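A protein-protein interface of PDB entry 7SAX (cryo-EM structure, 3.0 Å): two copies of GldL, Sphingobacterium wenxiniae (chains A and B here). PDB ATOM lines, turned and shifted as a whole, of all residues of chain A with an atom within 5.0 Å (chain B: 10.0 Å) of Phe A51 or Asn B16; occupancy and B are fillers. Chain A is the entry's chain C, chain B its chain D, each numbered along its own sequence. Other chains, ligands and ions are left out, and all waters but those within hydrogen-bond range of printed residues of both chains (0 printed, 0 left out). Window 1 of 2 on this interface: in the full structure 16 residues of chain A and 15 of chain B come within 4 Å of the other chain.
The backbone carbonyl oxygen of Asn B12 sits at hydrogen-bond distance from the side-chain amide nitrogen of Asn B16 (2.8 Å).
The backbone carbonyl oxygen (O) of Asn B16 sits at hydrogen-bond distance from the side-chain hydroxyl (OG1) of Thr B20, at 3.4 Å.
The backbone NH (N) of Ala B19 lies within hydrogen-bond range of the side-chain carboxylate (OE1) of Glu B47 (3.0 Å).
Hydrophobic or aromatic side chains of chain B that line the printed part of chain A: Trp B17, Ala B19 and Ile B23.
Printed residues of chain A that touch a printed residue of chain B: Glu A47, Ala A48, Phe A51, Phe A52, Gly A55 and Gln A58.
Hydrophobic or aromatic side chains of chain A within 4 Å of the printed part of chain B: Ala A48, Phe A51 and Phe A52.
Of the printed residues of chain B, Phe A51 touches Asn B16 (3.6 Å), Ala B19 (3.5 Å), Thr B20 (3.4 Å) and Ile B23 (3.4 Å).
Asn B16 touches three residues of chain A.
Printed residues of chain B within 4 Å of Ala A48: Thr B20 (3.1 Å) and Ile B23 (3.6 Å).
Of chain B, only Thr B13 and Asn B16 come within 4 Å of Gly A55.
Of the printed residues of chain B, Phe A52 touches Trp B17 (3.5 Å) and Thr B20 (3.0 Å).
Of the printed residues of chain B, Glu A47 touches Ile B23 (3.99 Å).
Ile A53 touches none of the printed residues of chain B.
Ile B24 touches none of the printed residues of chain A.
The nearest residue of chain B that does not touch Phe A51 is Trp B17 (4.6 Å).
The nearest printed residue of chain A that does not touch Ile B23 is Leu A49 (6.2 Å).
Glu A47 touches Ile B23.
Ile B23 touches Ala A48.
CB of Asn B16 touches O of Phe A51, at 3.6 Å.
CD1 of Phe A51 touches CB of Ala B19 (3.5 Å).
Thr B20 touches Phe A51.
Ile B23 touches Phe A51 (CD1 to CD2, 3.4 Å).
Gly A55 touches Asn B16 (CA to CB, 3.6 Å).
CB of Asn B12 touches NE2 of Gln A58, 3.2 Å away.
4 positions are printed for both chains.
The side-chain hydroxyl (OG1) of Thr B20 sits at hydrogen-bond distance from the backbone carbonyl oxygen (O) of Ala A48, at 3.1 Å.
O of Phe A52 sits at hydrogen-bond distance from NE1 of Trp B17, at 3.5 Å.
The side-chain hydroxyl of Thr B20 is in hydrogen-bond range of the backbone NH of Phe A52.
O of Gly A55 sits at hydrogen-bond distance from OG1 of Thr B13 (3.0 Å).
The side-chain amide nitrogen (ND2) of Asn B16 sits at hydrogen-bond distance from the side-chain amide oxygen (OE1) of Gln A58, 2.9 Å away.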
ATOM      1  N   GLU A  47       4.281  16.113  16.568  1.00  0.00           N
ATOM      2  CA  GLU A  47       5.085  17.322  16.467  1.00  0.00           C
ATOM      3  C   GLU A  47       5.013  17.921  15.071  1.00  0.00           C
ATOM      4  O   GLU A  47       5.053  19.145  14.918  1.00  0.00           O
ATOM      5  CB  GLU A  47       6.527  17.030  16.863  1.00  0.00           C
ATOM      6  CG  GLU A  47       7.371  18.262  16.821  1.00  0.00           C
ATOM      7  CD  GLU A  47       6.927  19.280  17.850  1.00  0.00           C
ATOM      8  OE1 GLU A  47       6.339  18.876  18.873  1.00  0.00           O
ATOM      9  OE2 GLU A  47       7.146  20.488  17.635  1.00  0.00           O
ATOM     10  N   ALA A  48       4.901  17.078  14.044  1.00  0.00           N
ATOM     11  CA  ALA A  48       4.632  17.579  12.701  1.00  0.00           C
ATOM     12  C   ALA A  48       3.290  18.290  12.649  1.00  0.00           C
ATOM     13  O   ALA A  48       3.155  19.339  12.011  1.00  0.00           O
ATOM     14  CB  ALA A  48       4.666  16.432  11.697  1.00  0.00           C
ATOM     15  N   LEU A  49       2.284  17.731  13.321  1.00  0.00           N
ATOM     16  CA  LEU A  49       0.984  18.384  13.351  1.00  0.00           C
ATOM     17  C   LEU A  49       1.060  19.748  14.028  1.00  0.00           C
ATOM     18  O   LEU A  49       0.426  20.704  13.574  1.00  0.00           O
ATOM     19  CB  LEU A  49      -0.037  17.498  14.051  1.00  0.00           C
ATOM     20  CG  LEU A  49      -1.436  18.098  14.081  1.00  0.00           C
ATOM     21  CD1 LEU A  49      -1.942  18.287  12.671  1.00  0.00           C
ATOM     22  CD2 LEU A  49      -2.375  17.214  14.869  1.00  0.00           C
ATOM     23  N   LEU A  50       1.813  19.862  15.122  1.00  0.00           N
ATOM     24  CA  LEU A  50       1.956  21.177  15.749  1.00  0.00           C
ATOM     25  C   LEU A  50       2.801  22.138  14.929  1.00  0.00           C
ATOM     26  O   LEU A  50       2.557  23.342  14.979  1.00  0.00           O
ATOM     27  CB  LEU A  50       2.513  21.087  17.167  1.00  0.00           C
ATOM     28  CG  LEU A  50       1.579  20.690  18.305  1.00  0.00           C
ATOM     29  CD1 LEU A  50       1.173  19.261  18.287  1.00  0.00           C
ATOM     30  CD2 LEU A  50       2.255  21.024  19.606  1.00  0.00           C
ATOM     31  N   PHE A  51       3.791  21.658  14.180  1.00  0.00           N
ATOM     32  CA  PHE A  51       4.473  22.558  13.253  1.00  0.00           C
ATOM     33  C   PHE A  51       3.509  23.096  12.208  1.00  0.00           C
ATOM     34  O   PHE A  51       3.525  24.288  11.894  1.00  0.00           O
ATOM     35  CB  PHE A  51       5.647  21.858  12.585  1.00  0.00           C
ATOM     36  CG  PHE A  51       6.943  22.036  13.304  1.00  0.00           C
ATOM     37  CD1 PHE A  51       7.697  23.167  13.103  1.00  0.00           C
ATOM     38  CD2 PHE A  51       7.418  21.072  14.158  1.00  0.00           C
ATOM     39  CE1 PHE A  51       8.887  23.338  13.747  1.00  0.00           C
ATOM     40  CE2 PHE A  51       8.614  21.240  14.805  1.00  0.00           C
ATOM     41  CZ  PHE A  51       9.348  22.370  14.598  1.00  0.00           C
ATOM     42  N   PHE A  52       2.647  22.233  11.676  1.00  0.00           N
ATOM     43  CA  PHE A  52       1.632  22.658  10.715  1.00  0.00           C
ATOM     44  C   PHE A  52       0.677  23.682  11.329  1.00  0.00           C
ATOM     45  O   PHE A  52       0.417  24.752  10.753  1.00  0.00           O
ATOM     46  CB  PHE A  52       0.899  21.402  10.239  1.00  0.00           C
ATOM     47  CG  PHE A  52      -0.023  21.605   9.084  1.00  0.00           C
ATOM     48  CD1 PHE A  52       0.219  20.963   7.890  1.00  0.00           C
ATOM     49  CD2 PHE A  52      -1.175  22.350   9.209  1.00  0.00           C
ATOM     50  CE1 PHE A  52      -0.630  21.117   6.827  1.00  0.00           C
ATOM     51  CE2 PHE A  52      -2.027  22.497   8.154  1.00  0.00           C
ATOM     52  CZ  PHE A  52      -1.756  21.885   6.960  1.00  0.00           C
ATOM     53  N   ILE A  53       0.155  23.374  12.515  1.00  0.00           N
ATOM     54  CA  ILE A  53      -0.801  24.253  13.175  1.00  0.00           C
ATOM     55  C   ILE A  53      -0.160  25.590  13.515  1.00  0.00           C
ATOM     56  O   ILE A  53      -0.781  26.645  13.359  1.00  0.00           O
ATOM     57  CB  ILE A  53      -1.378  23.565  14.423  1.00  0.00           C
ATOM     58  CG1 ILE A  53      -2.338  22.454  14.013  1.00  0.00           C
ATOM     59  CG2 ILE A  53      -2.087  24.563  15.301  1.00  0.00           C
ATOM     60  CD1 ILE A  53      -3.346  22.877  12.978  1.00  0.00           C
ATOM     61  N   MET A  54       1.080  25.573  14.005  1.00  0.00           N
ATOM     62  CA  MET A  54       1.783  26.811  14.294  1.00  0.00           C
ATOM     63  C   MET A  54       2.107  27.584  13.031  1.00  0.00           C
ATOM     64  O   MET A  54       2.154  28.813  13.075  1.00  0.00           O
ATOM     65  CB  MET A  54       3.062  26.521  15.073  1.00  0.00           C
ATOM     66  CG  MET A  54       2.822  26.116  16.515  1.00  0.00           C
ATOM     67  SD  MET A  54       1.430  26.976  17.267  1.00  0.00           S
ATOM     68  CE  MET A  54       2.109  28.620  17.471  1.00  0.00           C
ATOM     69  N   GLY A  55       2.320  26.898  11.911  1.00  0.00           N
ATOM     70  CA  GLY A  55       2.470  27.602  10.652  1.00  0.00           C
ATOM     71  C   GLY A  55       1.228  28.382  10.288  1.00  0.00           C
ATOM     72  O   GLY A  55       1.313  29.505   9.792  1.00  0.00           O
ATOM     73  N   GLN A  58       0.819  31.357  13.031  1.00  0.00           N
ATOM     74  CA  GLN A  58       1.792  32.426  12.898  1.00  0.00           C
ATOM     75  C   GLN A  58       1.419  33.412  11.800  1.00  0.00           C
ATOM     76  O   GLN A  58       1.958  34.523  11.770  1.00  0.00           O
ATOM     77  CB  GLN A  58       3.169  31.813  12.631  1.00  0.00           C
ATOM     78  CG  GLN A  58       4.313  32.789  12.560  1.00  0.00           C
ATOM     79  CD  GLN A  58       5.633  32.094  12.354  1.00  0.00           C
ATOM     80  OE1 GLN A  58       5.686  30.874  12.224  1.00  0.00           O
ATOM     81  NE2 GLN A  58       6.713  32.861  12.352  1.00  0.00           N
ATOM     82  N   GLY B  10       3.246  34.146   4.618  1.00  0.00           N
ATOM     83  CA  GLY B  10       4.536  34.713   4.308  1.00  0.00           C
ATOM     84  C   GLY B  10       5.582  33.632   4.141  1.00  0.00           C
ATOM     85  O   GLY B  10       5.293  32.506   3.746  1.00  0.00           O
ATOM     86  N   ILE B  11       6.821  34.002   4.449  1.00  0.00           N
ATOM     87  CA  ILE B  11       7.926  33.061   4.363  1.00  0.00           C
ATOM     88  C   ILE B  11       8.032  32.199   5.613  1.00  0.00           C
ATOM     89  O   ILE B  11       8.567  31.086   5.543  1.00  0.00           O
ATOM     90  CB  ILE B  11       9.239  33.821   4.109  1.00  0.00           C
ATOM     91  CG1 ILE B  11      10.379  32.862   3.798  1.00  0.00           C
ATOM     92  CG2 ILE B  11       9.587  34.691   5.297  1.00  0.00           C
ATOM     93  CD1 ILE B  11      10.294  32.291   2.426  1.00  0.00           C
ATOM     94  N   ASN B  12       7.520  32.671   6.750  1.00  0.00           N
ATOM     95  CA  ASN B  12       7.612  31.901   7.984  1.00  0.00           C
ATOM     96  C   ASN B  12       6.656  30.714   7.976  1.00  0.00           C
ATOM     97  O   ASN B  12       7.020  29.610   8.401  1.00  0.00           O
ATOM     98  CB  ASN B  12       7.330  32.806   9.176  1.00  0.00           C
ATOM     99  CG  ASN B  12       8.542  33.596   9.598  1.00  0.00           C
ATOM    100  OD1 ASN B  12       9.533  33.037  10.058  1.00  0.00           O
ATOM    101  ND2 ASN B  12       8.472  34.909   9.440  1.00  0.00           N
ATOM    102  N   THR B  13       5.425  30.926   7.513  1.00  0.00           N
ATOM    103  CA  THR B  13       4.487  29.820   7.384  1.00  0.00           C
ATOM    104  C   THR B  13       5.067  28.728   6.503  1.00  0.00           C
ATOM    105  O   THR B  13       4.929  27.532   6.793  1.00  0.00           O
ATOM    106  CB  THR B  13       3.169  30.325   6.802  1.00  0.00           C
ATOM    107  OG1 THR B  13       2.584  31.271   7.701  1.00  0.00           O
ATOM    108  CG2 THR B  13       2.207  29.181   6.589  1.00  0.00           C
ATOM    109  N   LEU B  14       5.744  29.126   5.432  1.00  0.00           N
ATOM    110  CA  LEU B  14       6.325  28.152   4.525  1.00  0.00           C
ATOM    111  C   LEU B  14       7.476  27.412   5.188  1.00  0.00           C
ATOM    112  O   LEU B  14       7.695  26.231   4.910  1.00  0.00           O
ATOM    113  CB  LEU B  14       6.763  28.860   3.249  1.00  0.00           C
ATOM    114  CG  LEU B  14       7.025  27.995   2.031  1.00  0.00           C
ATOM    115  CD1 LEU B  14       5.758  27.258   1.686  1.00  0.00           C
ATOM    116  CD2 LEU B  14       7.440  28.878   0.881  1.00  0.00           C
ATOM    117  N   ILE B  15       8.187  28.075   6.098  1.00  0.00           N
ATOM    118  CA  ILE B  15       9.231  27.413   6.876  1.00  0.00           C
ATOM    119  C   ILE B  15       8.635  26.349   7.781  1.00  0.00           C
ATOM    120  O   ILE B  15       9.146  25.228   7.874  1.00  0.00           O
ATOM    121  CB  ILE B  15      10.008  28.446   7.698  1.00  0.00           C
ATOM    122  CG1 ILE B  15      10.932  29.229   6.805  1.00  0.00           C
ATOM    123  CG2 ILE B  15      10.796  27.777   8.781  1.00  0.00           C
ATOM    124  CD1 ILE B  15      11.557  30.287   7.533  1.00  0.00           C
ATOM    125  N   ASN B  16       7.561  26.695   8.490  1.00  0.00           N
ATOM    126  CA  ASN B  16       6.951  25.727   9.391  1.00  0.00           C
ATOM    127  C   ASN B  16       6.399  24.539   8.619  1.00  0.00           C
ATOM    128  O   ASN B  16       6.483  23.396   9.076  1.00  0.00           O
ATOM    129  CB  ASN B  16       5.863  26.396  10.216  1.00  0.00           C
ATOM    130  CG  ASN B  16       6.426  27.290  11.282  1.00  0.00           C
ATOM    131  OD1 ASN B  16       6.626  26.868  12.415  1.00  0.00           O
ATOM    132  ND2 ASN B  16       6.699  28.532  10.927  1.00  0.00           N
ATOM    133  N   TRP B  17       5.843  24.782   7.436  1.00  0.00           N
ATOM    134  CA  TRP B  17       5.349  23.666   6.641  1.00  0.00           C
ATOM    135  C   TRP B  17       6.484  22.820   6.078  1.00  0.00           C
ATOM    136  O   TRP B  17       6.353  21.593   5.981  1.00  0.00           O
ATOM    137  CB  TRP B  17       4.448  24.190   5.536  1.00  0.00           C
ATOM    138  CG  TRP B  17       3.166  24.684   6.083  1.00  0.00           C
ATOM    139  CD1 TRP B  17       2.722  24.547   7.358  1.00  0.00           C
ATOM    140  CD2 TRP B  17       2.155  25.404   5.381  1.00  0.00           C
ATOM    141  NE1 TRP B  17       1.495  25.132   7.497  1.00  0.00           N
ATOM    142  CE2 TRP B  17       1.123  25.667   6.293  1.00  0.00           C
ATOM    143  CE3 TRP B  17       2.021  25.850   4.066  1.00  0.00           C
ATOM    144  CZ2 TRP B  17      -0.023  26.354   5.937  1.00  0.00           C
ATOM    145  CZ3 TRP B  17       0.885  26.530   3.716  1.00  0.00           C
ATOM    146  CH2 TRP B  17      -0.124  26.777   4.645  1.00  0.00           C
ATOM    147  N   GLY B  18       7.606  23.437   5.712  1.00  0.00           N
ATOM    148  CA  GLY B  18       8.772  22.646   5.361  1.00  0.00           C
ATOM    149  C   GLY B  18       9.231  21.774   6.512  1.00  0.00           C
ATOM    150  O   GLY B  18       9.604  20.615   6.322  1.00  0.00           O
ATOM    151  N   ALA B  19       9.193  22.320   7.727  1.00  0.00           N
ATOM    152  CA  ALA B  19       9.518  21.533   8.910  1.00  0.00           C
ATOM    153  C   ALA B  19       8.549  20.375   9.081  1.00  0.00           C
ATOM    154  O   ALA B  19       8.950  19.274   9.466  1.00  0.00           O
ATOM    155  CB  ALA B  19       9.507  22.424  10.148  1.00  0.00           C
ATOM    156  N   THR B  20       7.266  20.614   8.816  1.00  0.00           N
ATOM    157  CA  THR B  20       6.280  19.539   8.858  1.00  0.00           C
ATOM    158  C   THR B  20       6.648  18.419   7.896  1.00  0.00           C
ATOM    159  O   THR B  20       6.551  17.235   8.238  1.00  0.00           O
ATOM    160  CB  THR B  20       4.898  20.086   8.516  1.00  0.00           C
ATOM    161  OG1 THR B  20       4.382  20.818   9.629  1.00  0.00           O
ATOM    162  CG2 THR B  20       3.951  18.962   8.188  1.00  0.00           C
ATOM    163  N   VAL B  21       7.073  18.779   6.685  1.00  0.00           N
ATOM    164  CA  VAL B  21       7.481  17.766   5.712  1.00  0.00           C
ATOM    165  C   VAL B  21       8.695  16.992   6.215  1.00  0.00           C
ATOM    166  O   VAL B  21       8.753  15.759   6.113  1.00  0.00           O
ATOM    167  CB  VAL B  21       7.756  18.418   4.347  1.00  0.00           C
ATOM    168  CG1 VAL B  21       8.305  17.396   3.385  1.00  0.00           C
ATOM    169  CG2 VAL B  21       6.494  19.035   3.805  1.00  0.00           C
ATOM    170  N   VAL B  22       9.678  17.700   6.772  1.00  0.00           N
ATOM    171  CA  VAL B  22      10.867  17.031   7.295  1.00  0.00           C
ATOM    172  C   VAL B  22      10.491  16.055   8.395  1.00  0.00           C
ATOM    173  O   VAL B  22      11.029  14.949   8.476  1.00  0.00           O
ATOM    174  CB  VAL B  22      11.891  18.055   7.807  1.00  0.00           C
ATOM    175  CG1 VAL B  22      13.132  17.343   8.285  1.00  0.00           C
ATOM    176  CG2 VAL B  22      12.231  19.037   6.742  1.00  0.00           C
ATOM    177  N   ILE B  23       9.579  16.460   9.279  1.00  0.00           N
ATOM    178  CA  ILE B  23       9.229  15.623  10.419  1.00  0.00           C
ATOM    179  C   ILE B  23       8.408  14.423   9.989  1.00  0.00           C
ATOM    180  O   ILE B  23       8.522  13.344  10.579  1.00  0.00           O
ATOM    181  CB  ILE B  23       8.510  16.464  11.479  1.00  0.00           C
ATOM    182  CG1 ILE B  23       9.456  17.536  11.986  1.00  0.00           C
ATOM    183  CG2 ILE B  23       8.097  15.612  12.632  1.00  0.00           C
ATOM    184  CD1 ILE B  23       8.949  18.235  13.157  1.00  0.00           C
ATOM    185  N   ILE B  24       7.571  14.572   8.964  1.00  0.00           N
ATOM    186  CA  ILE B  24       6.897  13.405   8.406  1.00  0.00           C
ATOM    187  C   ILE B  24       7.918  12.446   7.814  1.00  0.00           C
ATOM    188  O   ILE B  24       7.803  11.224   7.959  1.00  0.00           O
ATOM    189  CB  ILE B  24       5.847  13.836   7.370  1.00  0.00           C
ATOM    190  CG1 ILE B  24       4.637  14.434   8.075  1.00  0.00           C
ATOM    191  CG2 ILE B  24       5.415  12.665   6.533  1.00  0.00           C
ATOM    192  CD1 ILE B  24       3.562  14.890   7.141  1.00  0.00           C
ATOM    193  N   LEU B  26      10.974  12.114   8.917  1.00  0.00           N
ATOM    194  CA  LEU B  26      11.629  11.506  10.072  1.00  0.00           C
ATOM    195  C   LEU B  26      10.779  10.392  10.662  1.00  0.00           C
ATOM    196  O   LEU B  26      11.298   9.339  11.043  1.00  0.00           O
ATOM    197  CB  LEU B  26      11.913  12.561  11.136  1.00  0.00           C
ATOM    198  CG  LEU B  26      12.833  13.724  10.792  1.00  0.00           C
ATOM    199  CD1 LEU B  26      12.860  14.717  11.925  1.00  0.00           C
ATOM    200  CD2 LEU B  26      14.217  13.224  10.495  1.00  0.00           C
ATOM    201  N   GLY B  43      12.543  18.146   2.164  1.00  0.00           N
ATOM    202  CA  GLY B  43      12.145  19.122   3.157  1.00  0.00           C
ATOM    203  C   GLY B  43      13.325  19.835   3.778  1.00  0.00           C
ATOM    204  O   GLY B  43      13.257  21.030   4.046  1.00  0.00           O
ATOM    205  N   VAL B  46      14.661  22.337   1.228  1.00  0.00           N
ATOM    206  CA  VAL B  46      13.757  23.475   1.117  1.00  0.00           C
ATOM    207  C   VAL B  46      13.838  24.347   2.362  1.00  0.00           C
ATOM    208  O   VAL B  46      13.806  25.577   2.276  1.00  0.00           O
ATOM    209  CB  VAL B  46      12.326  22.989   0.850  1.00  0.00           C
ATOM    210  CG1 VAL B  46      11.340  24.121   1.011  1.00  0.00           C
ATOM    211  CG2 VAL B  46      12.232  22.405  -0.538  1.00  0.00           C
ATOM    212  N   GLU B  47      13.954  23.730   3.537  1.00  0.00           N
ATOM    213  CA  GLU B  47      14.088  24.489   4.774  1.00  0.00           C
ATOM    214  C   GLU B  47      15.386  25.281   4.798  1.00  0.00           C
ATOM    215  O   GLU B  47      15.403  26.444   5.215  1.00  0.00           O
ATOM    216  CB  GLU B  47      14.013  23.541   5.964  1.00  0.00           C
ATOM    217  CG  GLU B  47      13.753  24.227   7.273  1.00  0.00           C
ATOM    218  CD  GLU B  47      12.286  24.352   7.567  1.00  0.00           C
ATOM    219  OE1 GLU B  47      11.475  23.973   6.701  1.00  0.00           O
ATOM    220  OE2 GLU B  47      11.936  24.827   8.664  1.00  0.00           O
ATOM    221  N   LEU B  50      14.947  28.221   2.429  1.00  0.00           N
ATOM    222  CA  LEU B  50      14.079  29.253   2.982  1.00  0.00           C
ATOM    223  C   LEU B  50      14.759  30.012   4.110  1.00  0.00           C
ATOM    224  O   LEU B  50      14.537  31.217   4.264  1.00  0.00           O
ATOM    225  CB  LEU B  50      12.774  28.638   3.474  1.00  0.00           C
ATOM    226  CG  LEU B  50      11.885  28.019   2.401  1.00  0.00           C
ATOM    227  CD1 LEU B  50      10.715  27.305   3.030  1.00  0.00           C
ATOM    228  CD2 LEU B  50      11.413  29.065   1.428  1.00  0.00           C
ATOM    229  N   PHE B  51      15.569  29.330   4.920  1.00  0.00           N
ATOM    230  CA  PHE B  51      16.330  30.027   5.949  1.00  0.00           C
ATOM    231  C   PHE B  51      17.390  30.921   5.332  1.00  0.00           C
ATOM    232  O   PHE B  51      17.657  32.015   5.837  1.00  0.00           O
ATOM    233  CB  PHE B  51      16.957  29.021   6.906  1.00  0.00           C
ATOM    234  CG  PHE B  51      16.085  28.680   8.062  1.00  0.00           C
ATOM    235  CD1 PHE B  51      15.728  29.646   8.973  1.00  0.00           C
ATOM    236  CD2 PHE B  51      15.603  27.404   8.228  1.00  0.00           C
ATOM    237  CE1 PHE B  51      14.920  29.346  10.028  1.00  0.00           C
ATOM    238  CE2 PHE B  51      14.795  27.098   9.285  1.00  0.00           C
ATOM    239  CZ  PHE B  51      14.452  28.070  10.185  1.00  0.00           C
ATOM    240  N   MET B  54      15.702  34.330   4.100  1.00  0.00           N
ATOM    241  CA  MET B  54      15.330  35.367   5.058  1.00  0.00           C
ATOM    242  C   MET B  54      16.524  36.151   5.563  1.00  0.00           C
ATOM    243  O   MET B  54      16.338  37.214   6.162  1.00  0.00           O
ATOM    244  CB  MET B  54      14.636  34.796   6.275  1.00  0.00           C
ATOM    245  CG  MET B  54      13.311  34.177   6.055  1.00  0.00           C
ATOM    246  SD  MET B  54      12.867  33.730   7.716  1.00  0.00           S
ATOM    247  CE  MET B  54      14.008  32.372   7.858  1.00  0.00           C
